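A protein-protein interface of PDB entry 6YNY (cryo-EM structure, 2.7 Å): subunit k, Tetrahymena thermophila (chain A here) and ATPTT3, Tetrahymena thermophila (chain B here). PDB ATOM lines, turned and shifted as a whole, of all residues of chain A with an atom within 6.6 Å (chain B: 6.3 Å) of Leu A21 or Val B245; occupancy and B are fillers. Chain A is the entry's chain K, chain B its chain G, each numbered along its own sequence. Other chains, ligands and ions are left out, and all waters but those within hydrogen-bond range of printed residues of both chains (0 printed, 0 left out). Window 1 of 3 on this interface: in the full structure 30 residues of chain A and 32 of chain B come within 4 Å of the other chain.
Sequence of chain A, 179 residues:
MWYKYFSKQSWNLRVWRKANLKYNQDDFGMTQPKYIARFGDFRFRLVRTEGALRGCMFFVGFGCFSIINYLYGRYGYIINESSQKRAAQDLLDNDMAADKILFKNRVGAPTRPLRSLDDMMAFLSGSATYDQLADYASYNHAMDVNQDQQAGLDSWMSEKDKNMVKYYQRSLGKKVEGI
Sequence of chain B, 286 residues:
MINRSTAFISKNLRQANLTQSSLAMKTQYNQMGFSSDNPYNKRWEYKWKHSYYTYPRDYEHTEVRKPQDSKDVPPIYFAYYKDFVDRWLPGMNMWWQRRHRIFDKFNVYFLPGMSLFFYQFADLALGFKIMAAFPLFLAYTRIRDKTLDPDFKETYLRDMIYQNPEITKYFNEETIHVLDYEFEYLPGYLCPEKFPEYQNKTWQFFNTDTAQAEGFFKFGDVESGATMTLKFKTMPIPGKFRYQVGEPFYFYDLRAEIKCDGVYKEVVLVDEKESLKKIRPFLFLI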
ATOM      1  N   LEU A  13      39.572  10.684   3.877  1.00  0.00           N
ATOM      2  CA  LEU A  13      38.273  10.432   3.281  1.00  0.00           C
ATOM      3  C   LEU A  13      37.473   9.493   4.171  1.00  0.00           C
ATOM      4  O   LEU A  13      38.023   8.761   4.997  1.00  0.00           O
ATOM      5  CB  LEU A  13      38.402   9.815   1.884  1.00  0.00           C
ATOM      6  CG  LEU A  13      39.373  10.457   0.896  1.00  0.00           C
ATOM      7  CD1 LEU A  13      39.292   9.735  -0.421  1.00  0.00           C
ATOM      8  CD2 LEU A  13      39.095  11.925   0.704  1.00  0.00           C
ATOM      9  N   ARG A  14      36.153   9.528   3.993  1.00  0.00           N
ATOM     10  CA  ARG A  14      35.229   8.589   4.624  1.00  0.00           C
ATOM     11  C   ARG A  14      34.424   7.969   3.488  1.00  0.00           C
ATOM     12  O   ARG A  14      33.364   8.476   3.113  1.00  0.00           O
ATOM     13  CB  ARG A  14      34.342   9.272   5.648  1.00  0.00           C
ATOM     14  CG  ARG A  14      33.372   8.346   6.356  1.00  0.00           C
ATOM     15  CD  ARG A  14      34.076   7.335   7.226  1.00  0.00           C
ATOM     16  NE  ARG A  14      33.134   6.434   7.884  1.00  0.00           N
ATOM     17  CZ  ARG A  14      32.745   5.260   7.397  1.00  0.00           C
ATOM     18  NH1 ARG A  14      33.210   4.819   6.240  1.00  0.00           N
ATOM     19  NH2 ARG A  14      31.884   4.520   8.073  1.00  0.00           N
ATOM     20  N   VAL A  15      34.938   6.879   2.938  1.00  0.00           N
ATOM     21  CA  VAL A  15      34.356   6.272   1.748  1.00  0.00           C
ATOM     22  C   VAL A  15      33.224   5.346   2.160  1.00  0.00           C
ATOM     23  O   VAL A  15      33.392   4.481   3.026  1.00  0.00           O
ATOM     24  CB  VAL A  15      35.427   5.521   0.944  1.00  0.00           C
ATOM     25  CG1 VAL A  15      34.819   4.864  -0.275  1.00  0.00           C
ATOM     26  CG2 VAL A  15      36.524   6.466   0.535  1.00  0.00           C
ATOM     27  N   TRP A  16      32.067   5.528   1.535  1.00  0.00           N
ATOM     28  CA  TRP A  16      30.911   4.678   1.784  1.00  0.00           C
ATOM     29  C   TRP A  16      30.075   4.656   0.516  1.00  0.00           C
ATOM     30  O   TRP A  16      29.627   5.708   0.052  1.00  0.00           O
ATOM     31  CB  TRP A  16      30.098   5.185   2.970  1.00  0.00           C
ATOM     32  CG  TRP A  16      29.029   4.252   3.399  1.00  0.00           C
ATOM     33  CD1 TRP A  16      29.194   3.068   4.044  1.00  0.00           C
ATOM     34  CD2 TRP A  16      27.622   4.422   3.227  1.00  0.00           C
ATOM     35  NE1 TRP A  16      27.979   2.485   4.280  1.00  0.00           N
ATOM     36  CE2 TRP A  16      26.995   3.299   3.788  1.00  0.00           C
ATOM     37  CE3 TRP A  16      26.829   5.416   2.651  1.00  0.00           C
ATOM     38  CZ2 TRP A  16      25.617   3.140   3.791  1.00  0.00           C
ATOM     39  CZ3 TRP A  16      25.465   5.256   2.653  1.00  0.00           C
ATOM     40  CH2 TRP A  16      24.872   4.129   3.219  1.00  0.00           C
ATOM     41  N   ALA A  19      31.534   6.734  -2.323  1.00  0.00           N
ATOM     42  CA  ALA A  19      31.378   8.170  -2.160  1.00  0.00           C
ATOM     43  C   ALA A  19      32.060   8.616  -0.880  1.00  0.00           C
ATOM     44  O   ALA A  19      32.012   7.916   0.136  1.00  0.00           O
ATOM     45  CB  ALA A  19      29.905   8.570  -2.121  1.00  0.00           C
ATOM     46  N   ASN A  20      32.694   9.781  -0.936  1.00  0.00           N
ATOM     47  CA  ASN A  20      33.325  10.378   0.230  1.00  0.00           C
ATOM     48  C   ASN A  20      32.298  11.227   0.965  1.00  0.00           C
ATOM     49  O   ASN A  20      31.747  12.174   0.395  1.00  0.00           O
ATOM     50  CB  ASN A  20      34.527  11.222  -0.179  1.00  0.00           C
ATOM     51  CG  ASN A  20      35.142  11.955   0.983  1.00  0.00           C
ATOM     52  OD1 ASN A  20      35.167  11.461   2.107  1.00  0.00           O
ATOM     53  ND2 ASN A  20      35.634  13.153   0.721  1.00  0.00           N
ATOM     54  N   LEU A  21      32.045  10.887   2.226  1.00  0.00           N
ATOM     55  CA  LEU A  21      31.064  11.619   3.011  1.00  0.00           C
ATOM     56  C   LEU A  21      31.561  12.998   3.417  1.00  0.00           C
ATOM     57  O   LEU A  21      30.748  13.851   3.783  1.00  0.00           O
ATOM     58  CB  LEU A  21      30.687  10.815   4.249  1.00  0.00           C
ATOM     59  CG  LEU A  21      30.235   9.381   3.984  1.00  0.00           C
ATOM     60  CD1 LEU A  21      29.860   8.694   5.268  1.00  0.00           C
ATOM     61  CD2 LEU A  21      29.080   9.347   3.025  1.00  0.00           C
ATOM     62  N   LYS A  22      32.868  13.233   3.364  1.00  0.00           N
ATOM     63  CA  LYS A  22      33.428  14.539   3.701  1.00  0.00           C
ATOM     64  C   LYS A  22      33.496  15.443   2.477  1.00  0.00           C
ATOM     65  O   LYS A  22      34.521  16.062   2.203  1.00  0.00           O
ATOM     66  CB  LYS A  22      34.814  14.366   4.307  1.00  0.00           C
ATOM     67  CG  LYS A  22      34.883  13.502   5.537  1.00  0.00           C
ATOM     68  CD  LYS A  22      36.316  13.411   6.031  1.00  0.00           C
ATOM     69  CE  LYS A  22      36.448  12.517   7.243  1.00  0.00           C
ATOM     70  NZ  LYS A  22      35.611  12.985   8.376  1.00  0.00           N
ATOM     71  N   TYR A  23      32.395  15.553   1.746  1.00  0.00           N
ATOM     72  CA  TYR A  23      32.331  16.373   0.546  1.00  0.00           C
ATOM     73  C   TYR A  23      31.383  17.535   0.791  1.00  0.00           C
ATOM     74  O   TYR A  23      30.220  17.329   1.149  1.00  0.00           O
ATOM     75  CB  TYR A  23      31.882  15.558  -0.663  1.00  0.00           C
ATOM     76  CG  TYR A  23      31.724  16.386  -1.913  1.00  0.00           C
ATOM     77  CD1 TYR A  23      32.818  16.991  -2.507  1.00  0.00           C
ATOM     78  CD2 TYR A  23      30.483  16.566  -2.497  1.00  0.00           C
ATOM     79  CE1 TYR A  23      32.680  17.752  -3.643  1.00  0.00           C
ATOM     80  CE2 TYR A  23      30.337  17.325  -3.634  1.00  0.00           C
ATOM     81  CZ  TYR A  23      31.439  17.917  -4.202  1.00  0.00           C
ATOM     82  OH  TYR A  23      31.300  18.673  -5.339  1.00  0.00           O
ATOM     83  N   ASN A  24      31.883  18.753   0.589  1.00  0.00           N
ATOM     84  CA  ASN A  24      31.107  19.965   0.825  1.00  0.00           C
ATOM     85  C   ASN A  24      30.136  20.174  -0.336  1.00  0.00           C
ATOM     86  O   ASN A  24      30.313  21.027  -1.207  1.00  0.00           O
ATOM     87  CB  ASN A  24      32.031  21.156   1.017  1.00  0.00           C
ATOM     88  CG  ASN A  24      31.308  22.377   1.517  1.00  0.00           C
ATOM     89  OD1 ASN A  24      30.109  22.341   1.782  1.00  0.00           O
ATOM     90  ND2 ASN A  24      32.039  23.468   1.666  1.00  0.00           N
ATOM     91  N   GLN A  25      29.083  19.357  -0.332  1.00  0.00           N
ATOM     92  CA  GLN A  25      28.030  19.487  -1.327  1.00  0.00           C
ATOM     93  C   GLN A  25      27.205  20.750  -1.138  1.00  0.00           C
ATOM     94  O   GLN A  25      26.447  21.114  -2.042  1.00  0.00           O
ATOM     95  CB  GLN A  25      27.116  18.263  -1.284  1.00  0.00           C
ATOM     96  CG  GLN A  25      26.472  18.007   0.062  1.00  0.00           C
ATOM     97  CD  GLN A  25      25.353  16.984   0.006  1.00  0.00           C
ATOM     98  OE1 GLN A  25      24.485  16.960   0.875  1.00  0.00           O
ATOM     99  NE2 GLN A  25      25.367  16.135  -1.010  1.00  0.00           N
ATOM    100  N   ARG A  48      20.853  11.846  -2.498  1.00  0.00           N
ATOM    101  CA  ARG A  48      21.854  12.344  -1.562  1.00  0.00           C
ATOM    102  C   ARG A  48      23.099  12.867  -2.268  1.00  0.00           C
ATOM    103  O   ARG A  48      23.982  13.437  -1.622  1.00  0.00           O
ATOM    104  CB  ARG A  48      22.270  11.252  -0.573  1.00  0.00           C
ATOM    105  CG  ARG A  48      21.140  10.438   0.006  1.00  0.00           C
ATOM    106  CD  ARG A  48      21.640   9.513   1.096  1.00  0.00           C
ATOM    107  NE  ARG A  48      22.850   8.804   0.704  1.00  0.00           N
ATOM    108  CZ  ARG A  48      22.872   7.713  -0.051  1.00  0.00           C
ATOM    109  NH1 ARG A  48      21.746   7.191  -0.511  1.00  0.00           N
ATOM    110  NH2 ARG A  48      24.027   7.143  -0.351  1.00  0.00           N
ATOM    111  N   PRO B 236      22.438   5.579  11.603  1.00  0.00           N
ATOM    112  CA  PRO B 236      22.968   6.603  10.702  1.00  0.00           C
ATOM    113  C   PRO B 236      22.529   7.992  11.125  1.00  0.00           C
ATOM    114  O   PRO B 236      21.392   8.198  11.555  1.00  0.00           O
ATOM    115  CB  PRO B 236      22.375   6.215   9.346  1.00  0.00           C
ATOM    116  CG  PRO B 236      21.133   5.508   9.680  1.00  0.00           C
ATOM    117  CD  PRO B 236      21.383   4.783  10.962  1.00  0.00           C
ATOM    118  N   ILE B 237      23.443   8.947  11.003  1.00  0.00           N
ATOM    119  CA  ILE B 237      23.176  10.320  11.421  1.00  0.00           C
ATOM    120  C   ILE B 237      23.552  11.261  10.286  1.00  0.00           C
ATOM    121  O   ILE B 237      24.387  10.929   9.430  1.00  0.00           O
ATOM    122  CB  ILE B 237      23.950  10.689  12.706  1.00  0.00           C
ATOM    123  CG1 ILE B 237      25.452  10.557  12.475  1.00  0.00           C
ATOM    124  CG2 ILE B 237      23.511   9.811  13.846  1.00  0.00           C
ATOM    125  CD1 ILE B 237      26.281  11.135  13.560  1.00  0.00           C
ATOM    126  N   PRO B 238      22.950  12.444  10.249  1.00  0.00           N
ATOM    127  CA  PRO B 238      23.387  13.474   9.308  1.00  0.00           C
ATOM    128  C   PRO B 238      24.535  14.297   9.860  1.00  0.00           C
ATOM    129  O   PRO B 238      24.646  14.536  11.064  1.00  0.00           O
ATOM    130  CB  PRO B 238      22.130  14.336   9.148  1.00  0.00           C
ATOM    131  CG  PRO B 238      21.464  14.231  10.464  1.00  0.00           C
ATOM    132  CD  PRO B 238      21.747  12.858  10.989  1.00  0.00           C
ATOM    133  N   GLY B 239      25.408  14.725   8.956  1.00  0.00           N
ATOM    134  CA  GLY B 239      26.525  15.546   9.366  1.00  0.00           C
ATOM    135  C   GLY B 239      26.901  16.663   8.417  1.00  0.00           C
ATOM    136  O   GLY B 239      27.242  16.426   7.256  1.00  0.00           O
ATOM    137  N   PHE B 241      25.935  18.608   6.425  1.00  0.00           N
ATOM    138  CA  PHE B 241      25.409  18.779   5.080  1.00  0.00           C
ATOM    139  C   PHE B 241      23.905  18.563   5.107  1.00  0.00           C
ATOM    140  O   PHE B 241      23.326  18.171   6.122  1.00  0.00           O
ATOM    141  CB  PHE B 241      26.084  17.834   4.084  1.00  0.00           C
ATOM    142  CG  PHE B 241      27.578  17.871   4.144  1.00  0.00           C
ATOM    143  CD1 PHE B 241      28.262  19.035   3.858  1.00  0.00           C
ATOM    144  CD2 PHE B 241      28.301  16.746   4.491  1.00  0.00           C
ATOM    145  CE1 PHE B 241      29.629  19.079   3.923  1.00  0.00           C
ATOM    146  CE2 PHE B 241      29.673  16.788   4.552  1.00  0.00           C
ATOM    147  CZ  PHE B 241      30.337  17.958   4.266  1.00  0.00           C
ATOM    148  N   TYR B 243      21.731  16.872   2.420  1.00  0.00           N
ATOM    149  CA  TYR B 243      21.137  15.653   1.891  1.00  0.00           C
ATOM    150  C   TYR B 243      21.939  14.398   2.195  1.00  0.00           C
ATOM    151  O   TYR B 243      21.357  13.314   2.288  1.00  0.00           O
ATOM    152  CB  TYR B 243      20.967  15.765   0.375  1.00  0.00           C
ATOM    153  CG  TYR B 243      20.263  17.016  -0.081  1.00  0.00           C
ATOM    154  CD1 TYR B 243      18.902  17.178   0.106  1.00  0.00           C
ATOM    155  CD2 TYR B 243      20.960  18.029  -0.718  1.00  0.00           C
ATOM    156  CE1 TYR B 243      18.258  18.317  -0.314  1.00  0.00           C
ATOM    157  CE2 TYR B 243      20.324  19.170  -1.142  1.00  0.00           C
ATOM    158  CZ  TYR B 243      18.972  19.309  -0.941  1.00  0.00           C
ATOM    159  OH  TYR B 243      18.335  20.448  -1.365  1.00  0.00           O
ATOM    160  N   GLN B 244      23.252  14.510   2.343  1.00  0.00           N
ATOM    161  CA  GLN B 244      24.110  13.349   2.502  1.00  0.00           C
ATOM    162  C   GLN B 244      24.230  12.945   3.965  1.00  0.00           C
ATOM    163  O   GLN B 244      24.188  13.782   4.871  1.00  0.00           O
ATOM    164  CB  GLN B 244      25.497  13.630   1.928  1.00  0.00           C
ATOM    165  CG  GLN B 244      26.454  12.461   1.982  1.00  0.00           C
ATOM    166  CD  GLN B 244      25.957  11.250   1.231  1.00  0.00           C
ATOM    167  OE1 GLN B 244      24.991  10.607   1.633  1.00  0.00           O
ATOM    168  NE2 GLN B 244      26.622  10.928   0.134  1.00  0.00           N
ATOM    169  N   VAL B 245      24.380  11.639   4.183  1.00  0.00           N
ATOM    170  CA  VAL B 245      24.577  11.119   5.526  1.00  0.00           C
ATOM    171  C   VAL B 245      25.986  11.447   6.000  1.00  0.00           C
ATOM    172  O   VAL B 245      26.937  11.511   5.209  1.00  0.00           O
ATOM    173  CB  VAL B 245      24.321   9.601   5.559  1.00  0.00           C
ATOM    174  CG1 VAL B 245      25.348   8.866   4.733  1.00  0.00           C
ATOM    175  CG2 VAL B 245      24.339   9.090   6.972  1.00  0.00           C
ATOM    176  N   GLY B 246      26.124  11.660   7.303  1.00  0.00           N
ATOM    177  CA  GLY B 246      27.418  11.963   7.875  1.00  0.00           C
ATOM    178  C   GLY B 246      28.186  10.720   8.261  1.00  0.00           C
ATOM    179  O   GLY B 246      29.361  10.569   7.914  1.00  0.00           O
ATOM    180  N   GLU B 247      27.528   9.823   8.982  1.00  0.00           N
ATOM    181  CA  GLU B 247      28.134   8.571   9.406  1.00  0.00           C
ATOM    182  C   GLU B 247      27.067   7.487   9.448  1.00  0.00           C
ATOM    183  O   GLU B 247      26.178   7.531  10.306  1.00  0.00           O
ATOM    184  CB  GLU B 247      28.799   8.716  10.774  1.00  0.00           C
ATOM    185  CG  GLU B 247      29.603   7.502  11.204  1.00  0.00           C
ATOM    186  CD  GLU B 247      30.894   7.332  10.420  1.00  0.00           C
ATOM    187  OE1 GLU B 247      30.848   7.327   9.175  1.00  0.00           O
ATOM    188  OE2 GLU B 247      31.961   7.199  11.055  1.00  0.00           O
ATOM    189  N   PRO B 248      27.108   6.505   8.545  1.00  0.00           N
ATOM    190  CA  PRO B 248      26.053   5.485   8.537  1.00  0.00           C
ATOM    191  C   PRO B 248      26.038   4.615   9.778  1.00  0.00           C
ATOM    192  O   PRO B 248      25.009   3.990  10.059  1.00  0.00           O
ATOM    193  CB  PRO B 248      26.371   4.662   7.284  1.00  0.00           C
ATOM    194  CG  PRO B 248      27.811   4.868   7.057  1.00  0.00           C
ATOM    195  CD  PRO B 248      28.113   6.255   7.499  1.00  0.00           C
ATOM    196  N   PHE B 282      18.931   9.270  10.389  1.00  0.00           N
ATOM    197  CA  PHE B 282      18.967   9.914   9.082  1.00  0.00           C
ATOM    198  C   PHE B 282      17.820   9.518   8.161  1.00  0.00           C
ATOM    199  O   PHE B 282      17.422  10.324   7.315  1.00  0.00           O
ATOM    200  CB  PHE B 282      20.290   9.601   8.385  1.00  0.00           C
ATOM    201  CG  PHE B 282      20.379  10.145   6.999  1.00  0.00           C
ATOM    202  CD1 PHE B 282      20.675  11.473   6.787  1.00  0.00           C
ATOM    203  CD2 PHE B 282      20.164   9.330   5.906  1.00  0.00           C
ATOM    204  CE1 PHE B 282      20.754  11.978   5.516  1.00  0.00           C
ATOM    205  CE2 PHE B 282      20.242   9.832   4.633  1.00  0.00           C
ATOM    206  CZ  PHE B 282      20.537  11.158   4.437  1.00  0.00           C
ATOM    207  N   PHE B 284      17.367   6.937   5.650  1.00  0.00           N
ATOM    208  CA  PHE B 284      17.732   6.728   4.256  1.00  0.00           C
ATOM    209  C   PHE B 284      16.500   6.624   3.367  1.00  0.00           C
ATOM    210  O   PHE B 284      15.495   6.011   3.733  1.00  0.00           O
ATOM    211  CB  PHE B 284      18.557   5.451   4.104  1.00  0.00           C
ATOM    212  CG  PHE B 284      19.982   5.590   4.524  1.00  0.00           C
ATOM    213  CD1 PHE B 284      20.425   5.038   5.709  1.00  0.00           C
ATOM    214  CD2 PHE B 284      20.885   6.261   3.730  1.00  0.00           C
ATOM    215  CE1 PHE B 284      21.736   5.160   6.091  1.00  0.00           C
ATOM    216  CE2 PHE B 284      22.195   6.387   4.109  1.00  0.00           C
ATOM    217  CZ  PHE B 284      22.622   5.835   5.292  1.00  0.00           C
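The backbone NH of Arg A14 sits at hydrogen-bond distance from the side-chain amide oxygen of Asn A20.
O of Arg A14 lies within hydrogen-bond range of N of Leu A21 (2.9 Å).
NE2 of Gln A25 is in hydrogen-bond range of O of Arg A48 (3.1 Å).
The backbone NH (N) of Phe B282 lies within hydrogen-bond range of the backbone carbonyl oxygen (O) of Pro B236, 2.9 Å away.
N of Gly B246 is in hydrogen-bond range of O of Ile B237.
O of Glu B247 lies within hydrogen-bond range of N of Ile B237 (3.2 Å).
The side-chain carboxylate of Glu B247 lies within salt-bridge range of the guanidinium group of Arg A14, 2.8 Å away.
The backbone NH (N) of Tyr B243 lies within hydrogen-bond range of the side-chain amide oxygen (OE1) of Gln A25, at 3.2 Å.
The backbone NH (N) of Gln B244 sits at hydrogen-bond distance from the side-chain amide oxygen (OE1) of Gln A25, at 3.1 Å.
The guanidinium group of Arg A48 is in hydrogen-bond range of the side-chain amide oxygen of Gln B244, 2.9 Å away.
Among the printed residues, pairs that only touch across the chains: Tyr A23 with Phe B241 (3.2 Å), Leu A21 with Phe B241 (3.2 Å), Leu A21 with Gly B246 (3.3 Å), Trp A16 with Phe B284 (3.5 Å), Asn A24 with Phe B241 (3.5 Å), Arg A48 with Tyr B243 (3.6 Å), Trp A16 with Pro B248 (3.7 Å), Gln A25 with Phe B241 (3.7 Å), Leu A21 with Pro B248 (3.7 Å), Leu A21 with Val B245 (3.7 Å) and Arg A48 with Phe B282 (3.8 Å).
Val B245 touches one residue of chain A.
Printed residues of chain A within 4 Å of Pro B248: Trp A16 and Leu A21.
Of the printed residues of chain B, Asn A24 touches Phe B241 (3.5 Å).
Printed residues of chain B within 4 Å of Gln A25: Phe B241, Tyr B243 and Gln B244.
Of the printed residues of chain A, Gln B244 touches Gln A25 and Arg A48.
The nearest residue of chain B that does not touch Leu A21 is Gln B244 (4.1 Å).
The nearest residue of chain A that does not touch Val B245 is Trp A16 (4.2 Å).
Of the 12 printed residues of chain A, 7 touch a printed residue of chain B.
Printed residues of chain A that touch a printed residue of chain B: Arg A14, Trp A16, Leu A21, Tyr A23, Asn A24, Gln A25 and Arg A48.
Hydrophobic or aromatic side chains of chain A within 4 Å of the printed part of chain B: Trp A16 and Leu A21.
Of the 13 printed residues of chain B, 9 touch a printed residue of chain A.
Hydrophobic or aromatic side chains of chain B that line the printed part of chain A: Phe B241, Tyr B243, Pro B248, Phe B282 and Phe B284.
Among the printed residues, 15 pairs touch across the chains.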
